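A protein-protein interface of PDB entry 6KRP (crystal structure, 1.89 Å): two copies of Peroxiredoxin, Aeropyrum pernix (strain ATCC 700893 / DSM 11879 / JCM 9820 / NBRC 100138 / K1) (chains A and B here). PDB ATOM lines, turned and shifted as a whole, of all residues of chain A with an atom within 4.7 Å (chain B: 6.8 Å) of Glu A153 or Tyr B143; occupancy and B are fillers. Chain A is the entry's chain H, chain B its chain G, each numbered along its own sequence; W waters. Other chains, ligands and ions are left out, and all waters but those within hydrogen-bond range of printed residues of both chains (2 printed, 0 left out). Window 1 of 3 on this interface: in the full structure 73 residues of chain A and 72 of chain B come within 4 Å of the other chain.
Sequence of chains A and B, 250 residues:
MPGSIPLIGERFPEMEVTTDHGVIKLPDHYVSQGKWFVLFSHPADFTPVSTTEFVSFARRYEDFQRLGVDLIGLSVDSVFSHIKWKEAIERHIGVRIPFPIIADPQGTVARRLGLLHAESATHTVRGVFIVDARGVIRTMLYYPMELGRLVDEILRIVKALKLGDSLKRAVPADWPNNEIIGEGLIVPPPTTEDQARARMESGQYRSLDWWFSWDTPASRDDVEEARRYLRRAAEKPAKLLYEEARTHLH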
ATOM      1  N   ILE A   8      26.275  10.088   0.476  1.00  0.00           N
ATOM      2  CA  ILE A   8      25.395   8.926   0.731  1.00  0.00           C
ATOM      3  C   ILE A   8      26.265   7.696   1.009  1.00  0.00           C
ATOM      4  O   ILE A   8      27.216   7.444   0.229  1.00  0.00           O
ATOM      5  CB  ILE A   8      24.410   8.707  -0.433  1.00  0.00           C
ATOM      6  CG1 ILE A   8      23.450   9.890  -0.567  1.00  0.00           C
ATOM      7  CG2 ILE A   8      23.693   7.382  -0.225  1.00  0.00           C
ATOM      8  CD1 ILE A   8      22.536   9.823  -1.766  1.00  0.00           C
ATOM      9  N   THR A 139      20.158   9.753   2.093  1.00  0.00           N
ATOM     10  CA  THR A 139      19.539  10.656   1.093  1.00  0.00           C
ATOM     11  C   THR A 139      19.883  12.093   1.488  1.00  0.00           C
ATOM     12  O   THR A 139      19.900  12.391   2.734  1.00  0.00           O
ATOM     13  CB  THR A 139      18.013  10.458   0.988  1.00  0.00           C
ATOM     14  OG1 THR A 139      17.737   9.258   0.296  1.00  0.00           O
ATOM     15  CG2 THR A 139      17.298  11.520   0.186  1.00  0.00           C
ATOM     16  N   LEU A 141      18.968  16.285   0.117  1.00  0.00           N
ATOM     17  CA  LEU A 141      18.163  17.186  -0.746  1.00  0.00           C
ATOM     18  C   LEU A 141      18.693  18.595  -0.529  1.00  0.00           C
ATOM     19  O   LEU A 141      18.979  18.942   0.646  1.00  0.00           O
ATOM     20  CB  LEU A 141      16.684  17.124  -0.356  1.00  0.00           C
ATOM     21  CG  LEU A 141      16.065  15.740  -0.163  1.00  0.00           C
ATOM     22  CD1 LEU A 141      14.665  15.911   0.390  1.00  0.00           C
ATOM     23  CD2 LEU A 141      16.074  14.945  -1.465  1.00  0.00           C
ATOM     24  N   LEU A 150       8.793  19.934   0.191  1.00  0.00           N
ATOM     25  CA  LEU A 150       7.553  19.107   0.252  1.00  0.00           C
ATOM     26  C   LEU A 150       7.781  18.085   1.336  1.00  0.00           C
ATOM     27  O   LEU A 150       8.527  17.136   1.085  1.00  0.00           O
ATOM     28  CB  LEU A 150       7.288  18.451  -1.098  1.00  0.00           C
ATOM     29  CG  LEU A 150       5.972  17.672  -1.170  1.00  0.00           C
ATOM     30  CD1 LEU A 150       4.807  18.654  -1.245  1.00  0.00           C
ATOM     31  CD2 LEU A 150       5.948  16.692  -2.334  1.00  0.00           C
ATOM     32  N   VAL A 151       7.251  18.332   2.525  1.00  0.00           N
ATOM     33  CA  VAL A 151       7.671  17.568   3.735  1.00  0.00           C
ATOM     34  C   VAL A 151       7.149  16.132   3.640  1.00  0.00           C
ATOM     35  O   VAL A 151       7.856  15.206   4.091  1.00  0.00           O
ATOM     36  CB  VAL A 151       7.283  18.298   5.029  1.00  0.00           C
ATOM     37  CG1 VAL A 151       7.726  17.534   6.262  1.00  0.00           C
ATOM     38  CG2 VAL A 151       7.923  19.674   5.052  1.00  0.00           C
ATOM     39  N   ASP A 152       6.027  15.910   2.949  1.00  0.00           N
ATOM     40  CA  ASP A 152       5.509  14.529   2.781  1.00  0.00           C
ATOM     41  C   ASP A 152       6.472  13.676   1.965  1.00  0.00           C
ATOM     42  O   ASP A 152       6.497  12.468   2.215  1.00  0.00           O
ATOM     43  CB  ASP A 152       4.083  14.524   2.251  1.00  0.00           C
ATOM     44  CG  ASP A 152       3.122  15.046   3.284  1.00  0.00           C
ATOM     45  OD1 ASP A 152       3.114  14.484   4.391  1.00  0.00           O
ATOM     46  OD2 ASP A 152       2.409  16.017   2.979  1.00  0.00           O
ATOM     47  N   GLU A 153       7.285  14.237   1.075  1.00  0.00           N
ATOM     48  CA  GLU A 153       8.284  13.399   0.343  1.00  0.00           C
ATOM     49  C   GLU A 153       9.344  12.901   1.338  1.00  0.00           C
ATOM     50  O   GLU A 153       9.892  11.780   1.163  1.00  0.00           O
ATOM     51  CB  GLU A 153       8.883  14.163  -0.844  1.00  0.00           C
ATOM     52  CG  GLU A 153      10.070  13.471  -1.508  1.00  0.00           C
ATOM     53  CD  GLU A 153       9.782  12.093  -2.079  1.00  0.00           C
ATOM     54  OE1 GLU A 153       8.634  11.642  -1.920  1.00  0.00           O
ATOM     55  OE2 GLU A 153      10.719  11.460  -2.648  1.00  0.00           O
ATOM     56  N   ILE A 154       9.658  13.688   2.369  1.00  0.00           N
ATOM     57  CA  ILE A 154      10.673  13.278   3.366  1.00  0.00           C
ATOM     58  C   ILE A 154      10.110  12.091   4.177  1.00  0.00           C
ATOM     59  O   ILE A 154      10.852  11.093   4.385  1.00  0.00           O
ATOM     60  CB  ILE A 154      11.155  14.458   4.235  1.00  0.00           C
ATOM     61  CG1 ILE A 154      11.875  15.491   3.371  1.00  0.00           C
ATOM     62  CG2 ILE A 154      12.011  13.905   5.371  1.00  0.00           C
ATOM     63  CD1 ILE A 154      12.083  16.869   4.046  1.00  0.00           C
ATOM     64  N   LEU A 155       8.834  12.124   4.551  1.00  0.00           N
ATOM     65  CA  LEU A 155       8.165  10.929   5.140  1.00  0.00           C
ATOM     66  C   LEU A 155       8.199   9.736   4.166  1.00  0.00           C
ATOM     67  O   LEU A 155       8.567   8.624   4.593  1.00  0.00           O
ATOM     68  CB  LEU A 155       6.719  11.249   5.536  1.00  0.00           C
ATOM     69  CG  LEU A 155       6.587  12.147   6.760  1.00  0.00           C
ATOM     70  CD1 LEU A 155       5.189  12.717   6.812  1.00  0.00           C
ATOM     71  CD2 LEU A 155       6.968  11.389   8.036  1.00  0.00           C
ATOM     72  N   ARG A 156       7.828   9.924   2.918  1.00  0.00           N
ATOM     73  CA  ARG A 156       7.807   8.773   1.979  1.00  0.00           C
ATOM     74  C   ARG A 156       9.232   8.180   1.900  1.00  0.00           C
ATOM     75  O   ARG A 156       9.396   6.955   1.920  1.00  0.00           O
ATOM     76  CB  ARG A 156       7.313   9.247   0.620  1.00  0.00           C
ATOM     77  CG  ARG A 156       7.061   8.129  -0.397  1.00  0.00           C
ATOM     78  CD  ARG A 156       6.841   8.663  -1.796  1.00  0.00           C
ATOM     79  NE  ARG A 156       8.145   8.994  -2.389  1.00  0.00           N
ATOM     80  CZ  ARG A 156       8.979   8.177  -3.027  1.00  0.00           C
ATOM     81  NH1 ARG A 156       8.672   6.903  -3.249  1.00  0.00           N
ATOM     82  NH2 ARG A 156      10.155   8.661  -3.415  1.00  0.00           N
ATOM     83  N   ILE A 157      10.257   9.023   1.775  1.00  0.00           N
ATOM     84  CA  ILE A 157      11.661   8.536   1.675  1.00  0.00           C
ATOM     85  C   ILE A 157      11.943   7.604   2.851  1.00  0.00           C
ATOM     86  O   ILE A 157      12.528   6.533   2.617  1.00  0.00           O
ATOM     87  CB  ILE A 157      12.660   9.705   1.573  1.00  0.00           C
ATOM     88  CG1 ILE A 157      12.543  10.375   0.200  1.00  0.00           C
ATOM     89  CG2 ILE A 157      14.107   9.250   1.866  1.00  0.00           C
ATOM     90  CD1 ILE A 157      13.117  11.787   0.100  1.00  0.00           C
ATOM     91  N   GLU B  53      12.226   4.645 -13.226  1.00  0.00           N
ATOM     92  CA  GLU B  53      12.400   6.118 -13.268  1.00  0.00           C
ATOM     93  C   GLU B  53      12.386   6.622 -14.714  1.00  0.00           C
ATOM     94  O   GLU B  53      11.772   7.670 -14.972  1.00  0.00           O
ATOM     95  CB  GLU B  53      13.671   6.531 -12.544  1.00  0.00           C
ATOM     96  CG  GLU B  53      13.647   6.165 -11.068  1.00  0.00           C
ATOM     97  CD  GLU B  53      14.936   6.552 -10.388  1.00  0.00           C
ATOM     98  OE1 GLU B  53      15.994   6.182 -10.935  1.00  0.00           O
ATOM     99  OE2 GLU B  53      14.871   7.231  -9.312  1.00  0.00           O
ATOM    100  N   GLU B 119      28.222   4.662  -1.341  1.00  0.00           N
ATOM    101  CA  GLU B 119      27.389   3.444  -1.516  1.00  0.00           C
ATOM    102  C   GLU B 119      27.934   2.602  -2.682  1.00  0.00           C
ATOM    103  O   GLU B 119      27.858   1.374  -2.610  1.00  0.00           O
ATOM    104  CB  GLU B 119      25.941   3.927  -1.699  1.00  0.00           C
ATOM    105  CG  GLU B 119      24.910   2.862  -1.552  1.00  0.00           C
ATOM    106  CD  GLU B 119      23.470   3.373  -1.553  1.00  0.00           C
ATOM    107  OE1 GLU B 119      23.115   4.222  -2.397  1.00  0.00           O
ATOM    108  OE2 GLU B 119      22.718   2.865  -0.772  1.00  0.00           O
ATOM    109  N   THR B 124      27.125   5.884 -10.305  1.00  0.00           N
ATOM    110  CA  THR B 124      26.587   7.129  -9.741  1.00  0.00           C
ATOM    111  C   THR B 124      25.401   6.822  -8.833  1.00  0.00           C
ATOM    112  O   THR B 124      24.619   5.887  -9.157  1.00  0.00           O
ATOM    113  CB  THR B 124      26.105   8.098 -10.822  1.00  0.00           C
ATOM    114  OG1 THR B 124      25.548   9.204 -10.126  1.00  0.00           O
ATOM    115  CG2 THR B 124      25.053   7.530 -11.731  1.00  0.00           C
ATOM    116  N   VAL B 125      25.188   7.725  -7.878  1.00  0.00           N
ATOM    117  CA  VAL B 125      23.916   7.865  -7.126  1.00  0.00           C
ATOM    118  C   VAL B 125      22.816   8.342  -8.095  1.00  0.00           C
ATOM    119  O   VAL B 125      23.072   8.481  -9.349  1.00  0.00           O
ATOM    120  CB  VAL B 125      24.080   8.801  -5.909  1.00  0.00           C
ATOM    121  CG1 VAL B 125      25.112   8.266  -4.933  1.00  0.00           C
ATOM    122  CG2 VAL B 125      24.419  10.200  -6.330  1.00  0.00           C
ATOM    123  N   ARG B 126      21.615   8.545  -7.540  1.00  0.00           N
ATOM    124  CA  ARG B 126      20.441   9.030  -8.312  1.00  0.00           C
ATOM    125  C   ARG B 126      20.386  10.537  -8.078  1.00  0.00           C
ATOM    126  O   ARG B 126      19.564  11.015  -7.298  1.00  0.00           O
ATOM    127  CB  ARG B 126      19.140   8.327  -7.905  1.00  0.00           C
ATOM    128  CG  ARG B 126      19.101   6.826  -8.130  1.00  0.00           C
ATOM    129  CD  ARG B 126      17.754   6.188  -7.734  1.00  0.00           C
ATOM    130  NE  ARG B 126      18.025   4.776  -7.703  1.00  0.00           N
ATOM    131  CZ  ARG B 126      18.185   3.988  -8.776  1.00  0.00           C
ATOM    132  NH1 ARG B 126      18.606   2.753  -8.614  1.00  0.00           N
ATOM    133  NH2 ARG B 126      17.944   4.414  -9.990  1.00  0.00           N
ATOM    134  N   GLY B 127      21.293  11.268  -8.712  1.00  0.00           N
ATOM    135  CA  GLY B 127      21.352  12.724  -8.581  1.00  0.00           C
ATOM    136  C   GLY B 127      20.390  13.413  -9.539  1.00  0.00           C
ATOM    137  O   GLY B 127      19.998  12.828 -10.571  1.00  0.00           O
ATOM    138  N   VAL B 128      19.969  14.626  -9.174  1.00  0.00           N
ATOM    139  CA  VAL B 128      19.106  15.506  -9.990  1.00  0.00           C
ATOM    140  C   VAL B 128      19.660  16.921  -9.921  1.00  0.00           C
ATOM    141  O   VAL B 128      19.697  17.494  -8.793  1.00  0.00           O
ATOM    142  CB  VAL B 128      17.634  15.520  -9.530  1.00  0.00           C
ATOM    143  CG1 VAL B 128      16.779  16.363 -10.481  1.00  0.00           C
ATOM    144  CG2 VAL B 128      17.048  14.126  -9.386  1.00  0.00           C
ATOM    145  N   LEU B 141      19.053  17.232  -5.923  1.00  0.00           N
ATOM    146  CA  LEU B 141      18.533  16.082  -5.143  1.00  0.00           C
ATOM    147  C   LEU B 141      19.498  14.916  -5.315  1.00  0.00           C
ATOM    148  O   LEU B 141      20.004  14.713  -6.452  1.00  0.00           O
ATOM    149  CB  LEU B 141      17.133  15.703  -5.630  1.00  0.00           C
ATOM    150  CG  LEU B 141      16.123  16.830  -5.838  1.00  0.00           C
ATOM    151  CD1 LEU B 141      14.907  16.280  -6.551  1.00  0.00           C
ATOM    152  CD2 LEU B 141      15.732  17.481  -4.496  1.00  0.00           C
ATOM    153  N   TYR B 142      19.697  14.150  -4.251  1.00  0.00           N
ATOM    154  CA  TYR B 142      20.603  12.981  -4.205  1.00  0.00           C
ATOM    155  C   TYR B 142      19.869  11.843  -3.507  1.00  0.00           C
ATOM    156  O   TYR B 142      19.781  11.797  -2.267  1.00  0.00           O
ATOM    157  CB  TYR B 142      21.946  13.243  -3.521  1.00  0.00           C
ATOM    158  CG  TYR B 142      22.754  14.301  -4.223  1.00  0.00           C
ATOM    159  CD1 TYR B 142      23.593  13.992  -5.285  1.00  0.00           C
ATOM    160  CD2 TYR B 142      22.600  15.632  -3.864  1.00  0.00           C
ATOM    161  CE1 TYR B 142      24.299  14.983  -5.948  1.00  0.00           C
ATOM    162  CE2 TYR B 142      23.288  16.629  -4.524  1.00  0.00           C
ATOM    163  CZ  TYR B 142      24.155  16.298  -5.547  1.00  0.00           C
ATOM    164  OH  TYR B 142      24.812  17.280  -6.210  1.00  0.00           O
ATOM    165  N   TYR B 143      19.275  10.989  -4.341  1.00  0.00           N
ATOM    166  CA  TYR B 143      18.619   9.731  -3.911  1.00  0.00           C
ATOM    167  C   TYR B 143      19.620   8.585  -4.063  1.00  0.00           C
ATOM    168  O   TYR B 143      20.545   8.652  -4.878  1.00  0.00           O
ATOM    169  CB  TYR B 143      17.356   9.506  -4.733  1.00  0.00           C
ATOM    170  CG  TYR B 143      16.160  10.361  -4.357  1.00  0.00           C
ATOM    171  CD1 TYR B 143      16.168  11.738  -4.528  1.00  0.00           C
ATOM    172  CD2 TYR B 143      14.990   9.777  -3.902  1.00  0.00           C
ATOM    173  CE1 TYR B 143      15.049  12.516  -4.229  1.00  0.00           C
ATOM    174  CE2 TYR B 143      13.870  10.540  -3.589  1.00  0.00           C
ATOM    175  CZ  TYR B 143      13.910  11.918  -3.732  1.00  0.00           C
ATOM    176  OH  TYR B 143      12.807  12.670  -3.441  1.00  0.00           O
ATOM    177  N   PRO B 144      19.458   7.498  -3.270  1.00  0.00           N
ATOM    178  CA  PRO B 144      20.392   6.385  -3.279  1.00  0.00           C
ATOM    179  C   PRO B 144      19.998   5.268  -4.254  1.00  0.00           C
ATOM    180  O   PRO B 144      18.931   5.314  -4.857  1.00  0.00           O
ATOM    181  CB  PRO B 144      20.294   5.972  -1.802  1.00  0.00           C
ATOM    182  CG  PRO B 144      18.815   6.089  -1.509  1.00  0.00           C
ATOM    183  CD  PRO B 144      18.416   7.353  -2.243  1.00  0.00           C
ATOM    184  N   MET B 145      20.854   4.280  -4.380  1.00  0.00           N
ATOM    185  CA  MET B 145      20.640   3.131  -5.320  1.00  0.00           C
ATOM    186  C   MET B 145      19.294   2.459  -5.044  1.00  0.00           C
ATOM    187  O   MET B 145      18.587   2.070  -6.007  1.00  0.00           O
ATOM    188  CB  MET B 145      21.699   2.050  -5.114  1.00  0.00           C
ATOM    189  CG  MET B 145      23.089   2.519  -5.225  1.00  0.00           C
ATOM    190  SD  MET B 145      23.267   3.758  -6.529  1.00  0.00           S
ATOM    191  CE  MET B 145      25.034   3.638  -6.817  1.00  0.00           C
ATOM    192  N   GLU B 146      18.936   2.327  -3.781  1.00  0.00           N
ATOM    193  CA  GLU B 146      17.809   1.470  -3.352  1.00  0.00           C
ATOM    194  C   GLU B 146      16.432   2.168  -3.459  1.00  0.00           C
ATOM    195  O   GLU B 146      15.416   1.475  -3.232  1.00  0.00           O
ATOM    196  CB  GLU B 146      18.081   0.914  -1.954  1.00  0.00           C
ATOM    197  CG  GLU B 146      18.159   1.955  -0.847  1.00  0.00           C
ATOM    198  CD  GLU B 146      19.540   2.534  -0.546  1.00  0.00           C
ATOM    199  OE1 GLU B 146      19.702   3.042   0.566  1.00  0.00           O
ATOM    200  OE2 GLU B 146      20.442   2.482  -1.426  1.00  0.00           O
ATOM    201  N   LEU B 147      16.340   3.446  -3.852  1.00  0.00           N
ATOM    202  CA  LEU B 147      15.083   4.229  -3.718  1.00  0.00           C
ATOM    203  C   LEU B 147      14.862   5.031  -4.991  1.00  0.00           C
ATOM    204  O   LEU B 147      15.643   5.975  -5.248  1.00  0.00           O
ATOM    205  CB  LEU B 147      15.254   5.204  -2.552  1.00  0.00           C
ATOM    206  CG  LEU B 147      14.055   5.629  -1.720  1.00  0.00           C
ATOM    207  CD1 LEU B 147      14.187   7.073  -1.282  1.00  0.00           C
ATOM    208  CD2 LEU B 147      12.694   5.310  -2.279  1.00  0.00           C
ATOM    209  N   GLY B 148      13.750   4.812  -5.650  1.00  0.00           N
ATOM    210  CA  GLY B 148      13.351   5.593  -6.823  1.00  0.00           C
ATOM    211  C   GLY B 148      12.914   6.985  -6.406  1.00  0.00           C
ATOM    212  O   GLY B 148      12.390   7.154  -5.296  1.00  0.00           O
ATOM    213  N   ARG B 149      13.063   7.940  -7.329  1.00  0.00           N
ATOM    214  CA  ARG B 149      12.615   9.336  -7.170  1.00  0.00           C
ATOM    215  C   ARG B 149      11.088   9.459  -7.292  1.00  0.00           C
ATOM    216  O   ARG B 149      10.389   8.506  -7.698  1.00  0.00           O
ATOM    217  CB  ARG B 149      13.429  10.192  -8.138  1.00  0.00           C
ATOM    218  CG  ARG B 149      14.864  10.410  -7.673  1.00  0.00           C
ATOM    219  CD  ARG B 149      15.844  10.817  -8.766  1.00  0.00           C
ATOM    220  NE  ARG B 149      16.211   9.663  -9.588  1.00  0.00           N
ATOM    221  CZ  ARG B 149      17.295   9.594 -10.366  1.00  0.00           C
ATOM    222  NH1 ARG B 149      18.094  10.644 -10.458  1.00  0.00           N
ATOM    223  NH2 ARG B 149      17.555   8.516 -11.076  1.00  0.00           N
ATOM    224  N   LEU B 150      10.564  10.562  -6.767  1.00  0.00           N
ATOM    225  CA  LEU B 150       9.139  10.956  -6.906  1.00  0.00           C
ATOM    226  C   LEU B 150       9.134  12.014  -7.996  1.00  0.00           C
ATOM    227  O   LEU B 150       9.469  13.162  -7.698  1.00  0.00           O
ATOM    228  CB  LEU B 150       8.614  11.537  -5.594  1.00  0.00           C
ATOM    229  CG  LEU B 150       7.102  11.770  -5.566  1.00  0.00           C
ATOM    230  CD1 LEU B 150       6.367  10.430  -5.477  1.00  0.00           C
ATOM    231  CD2 LEU B 150       6.700  12.702  -4.429  1.00  0.00           C
ATOM    232  N   GLU B 153       7.421  15.552  -7.880  1.00  0.00           N
ATOM    233  CA  GLU B 153       8.040  16.632  -7.062  1.00  0.00           C
ATOM    234  C   GLU B 153       8.987  17.454  -7.950  1.00  0.00           C
ATOM    235  O   GLU B 153       9.034  18.662  -7.745  1.00  0.00           O
ATOM    236  CB  GLU B 153       8.740  16.075  -5.835  1.00  0.00           C
ATOM    237  CG  GLU B 153       9.576  17.113  -5.089  1.00  0.00           C
ATOM    238  CD  GLU B 153       8.791  18.301  -4.528  1.00  0.00           C
ATOM    239  OE1 GLU B 153       7.580  18.400  -4.788  1.00  0.00           O
ATOM    240  OE2 GLU B 153       9.420  19.203  -3.907  1.00  0.00           O
ATOM    241  N   ASP B 174       5.106  22.917   0.855  1.00  0.00           N
ATOM    242  CA  ASP B 174       3.918  22.081   0.473  1.00  0.00           C
ATOM    243  C   ASP B 174       2.988  22.865  -0.452  1.00  0.00           C
ATOM    244  O   ASP B 174       1.838  22.421  -0.677  1.00  0.00           O
ATOM    245  CB  ASP B 174       3.195  21.585   1.721  1.00  0.00           C
ATOM    246  CG  ASP B 174       4.134  21.040   2.786  1.00  0.00           C
ATOM    247  OD1 ASP B 174       4.998  20.232   2.460  1.00  0.00           O
ATOM    248  OD2 ASP B 174       3.968  21.428   3.948  1.00  0.00           O
HETATM  249  O   HOH W   1       4.157  17.681   1.859  1.00  0.00           O
HETATM  250  O   HOH W   2      10.572   5.222  -4.530  1.00  0.00           O
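The backbone NH of Val B128 sits at hydrogen-bond distance from the backbone carbonyl oxygen of Leu B141 (2.7 Å).
O of Tyr B143 is in hydrogen-bond range of N of Arg B126.
The guanidinium group of Arg B126 is in hydrogen-bond range of the backbone carbonyl oxygen of Pro B144 (3.0 Å).
The backbone NH (N) of Met B145 lies within hydrogen-bond range of the side-chain carboxylate (OE1) of Glu B119, at 3.0 Å.
The side-chain carboxylate (OE1) of Glu A153 is in salt-bridge range of the guanidinium group (NE) of Arg A156 (2.7 Å).
Printed residues of chain B within 4 Å of Ile A8: Glu B119, Tyr B142 and Tyr B143.
Of the printed residues of chain B, Glu A153 touches Tyr B143 and Leu B150.
Tyr B143 touches four residues of chain A.
Of the printed residues of chain A, Gly B148 touches Arg A156.
The nearest residue of chain B that does not touch Glu A153 is Arg B149 (5.1 Å).
The nearest residue of chain A that does not touch Tyr B143 is Arg A156 (4.2 Å).
Water W1 lies within hydrogen-bond range of OD2 of Asp A152 (2.7 Å), OD1 of Asp B174 (2.8 Å) and N of Val A151 (3.2 Å).
Water W2 lies within hydrogen-bond range of the backbone carbonyl oxygen of Gly B148 (2.8 Å) and the guanidinium group of Arg A156 (2.8 Å).
Leu B141 touches its own counterpart, Leu A141.
Leu A150 touches Glu B153, and with the chains exchanged Glu A153 touches Leu B150.
3 positions are printed for both chains.
Hydrophobic or aromatic side chains of chain A that line the printed part of chain B: Ile A8, Leu A141, Leu A150, Val A151 and Ile A157.
Printed residues of chain B that touch a printed residue of chain A: Glu B119, Leu B141, Tyr B142, Tyr B143, Pro B144, Leu B147, Gly B148, Leu B150, Glu B153 and Asp B174.
Hydrophobic or aromatic side chains of chain B within 4 Å of the printed part of chain A: Leu B141, Tyr B142, Tyr B143, Pro B144, Leu B147 and Leu B150.
Among the printed residues, 16 pairs touch across the chains.
The backbone carbonyl oxygen (O) of Gly B148 lies within hydrogen-bond range of the guanidinium group (NH2) of Arg A156 (3.3 Å).
The side-chain hydroxyl of Tyr B143 is in hydrogen-bond range of the side-chain carboxylate of Glu A153, at 2.5 Å.
N of Val A151 lies within hydrogen-bond range of OD1 of Asp B174 (2.9 Å).
The backbone carbonyl oxygen (O) of Ile A8 sits at hydrogen-bond distance from the backbone NH (N) of Glu B119, 3.3 Å away.
Among the printed residues, merely in contact across the chains: Thr A139 with Pro B144, Glu A153 with Leu B150, Leu A150 with Glu B153, Ile A8 with Tyr B142, Thr A139 with Tyr B142, Leu A150 with Asp B174, Ile A157 with Tyr B143, Leu A141 with Tyr B143, Ile A157 with Leu B147, Arg A156 with Leu B150, Ile A8 with Tyr B143 and Leu A141 with Leu B141.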
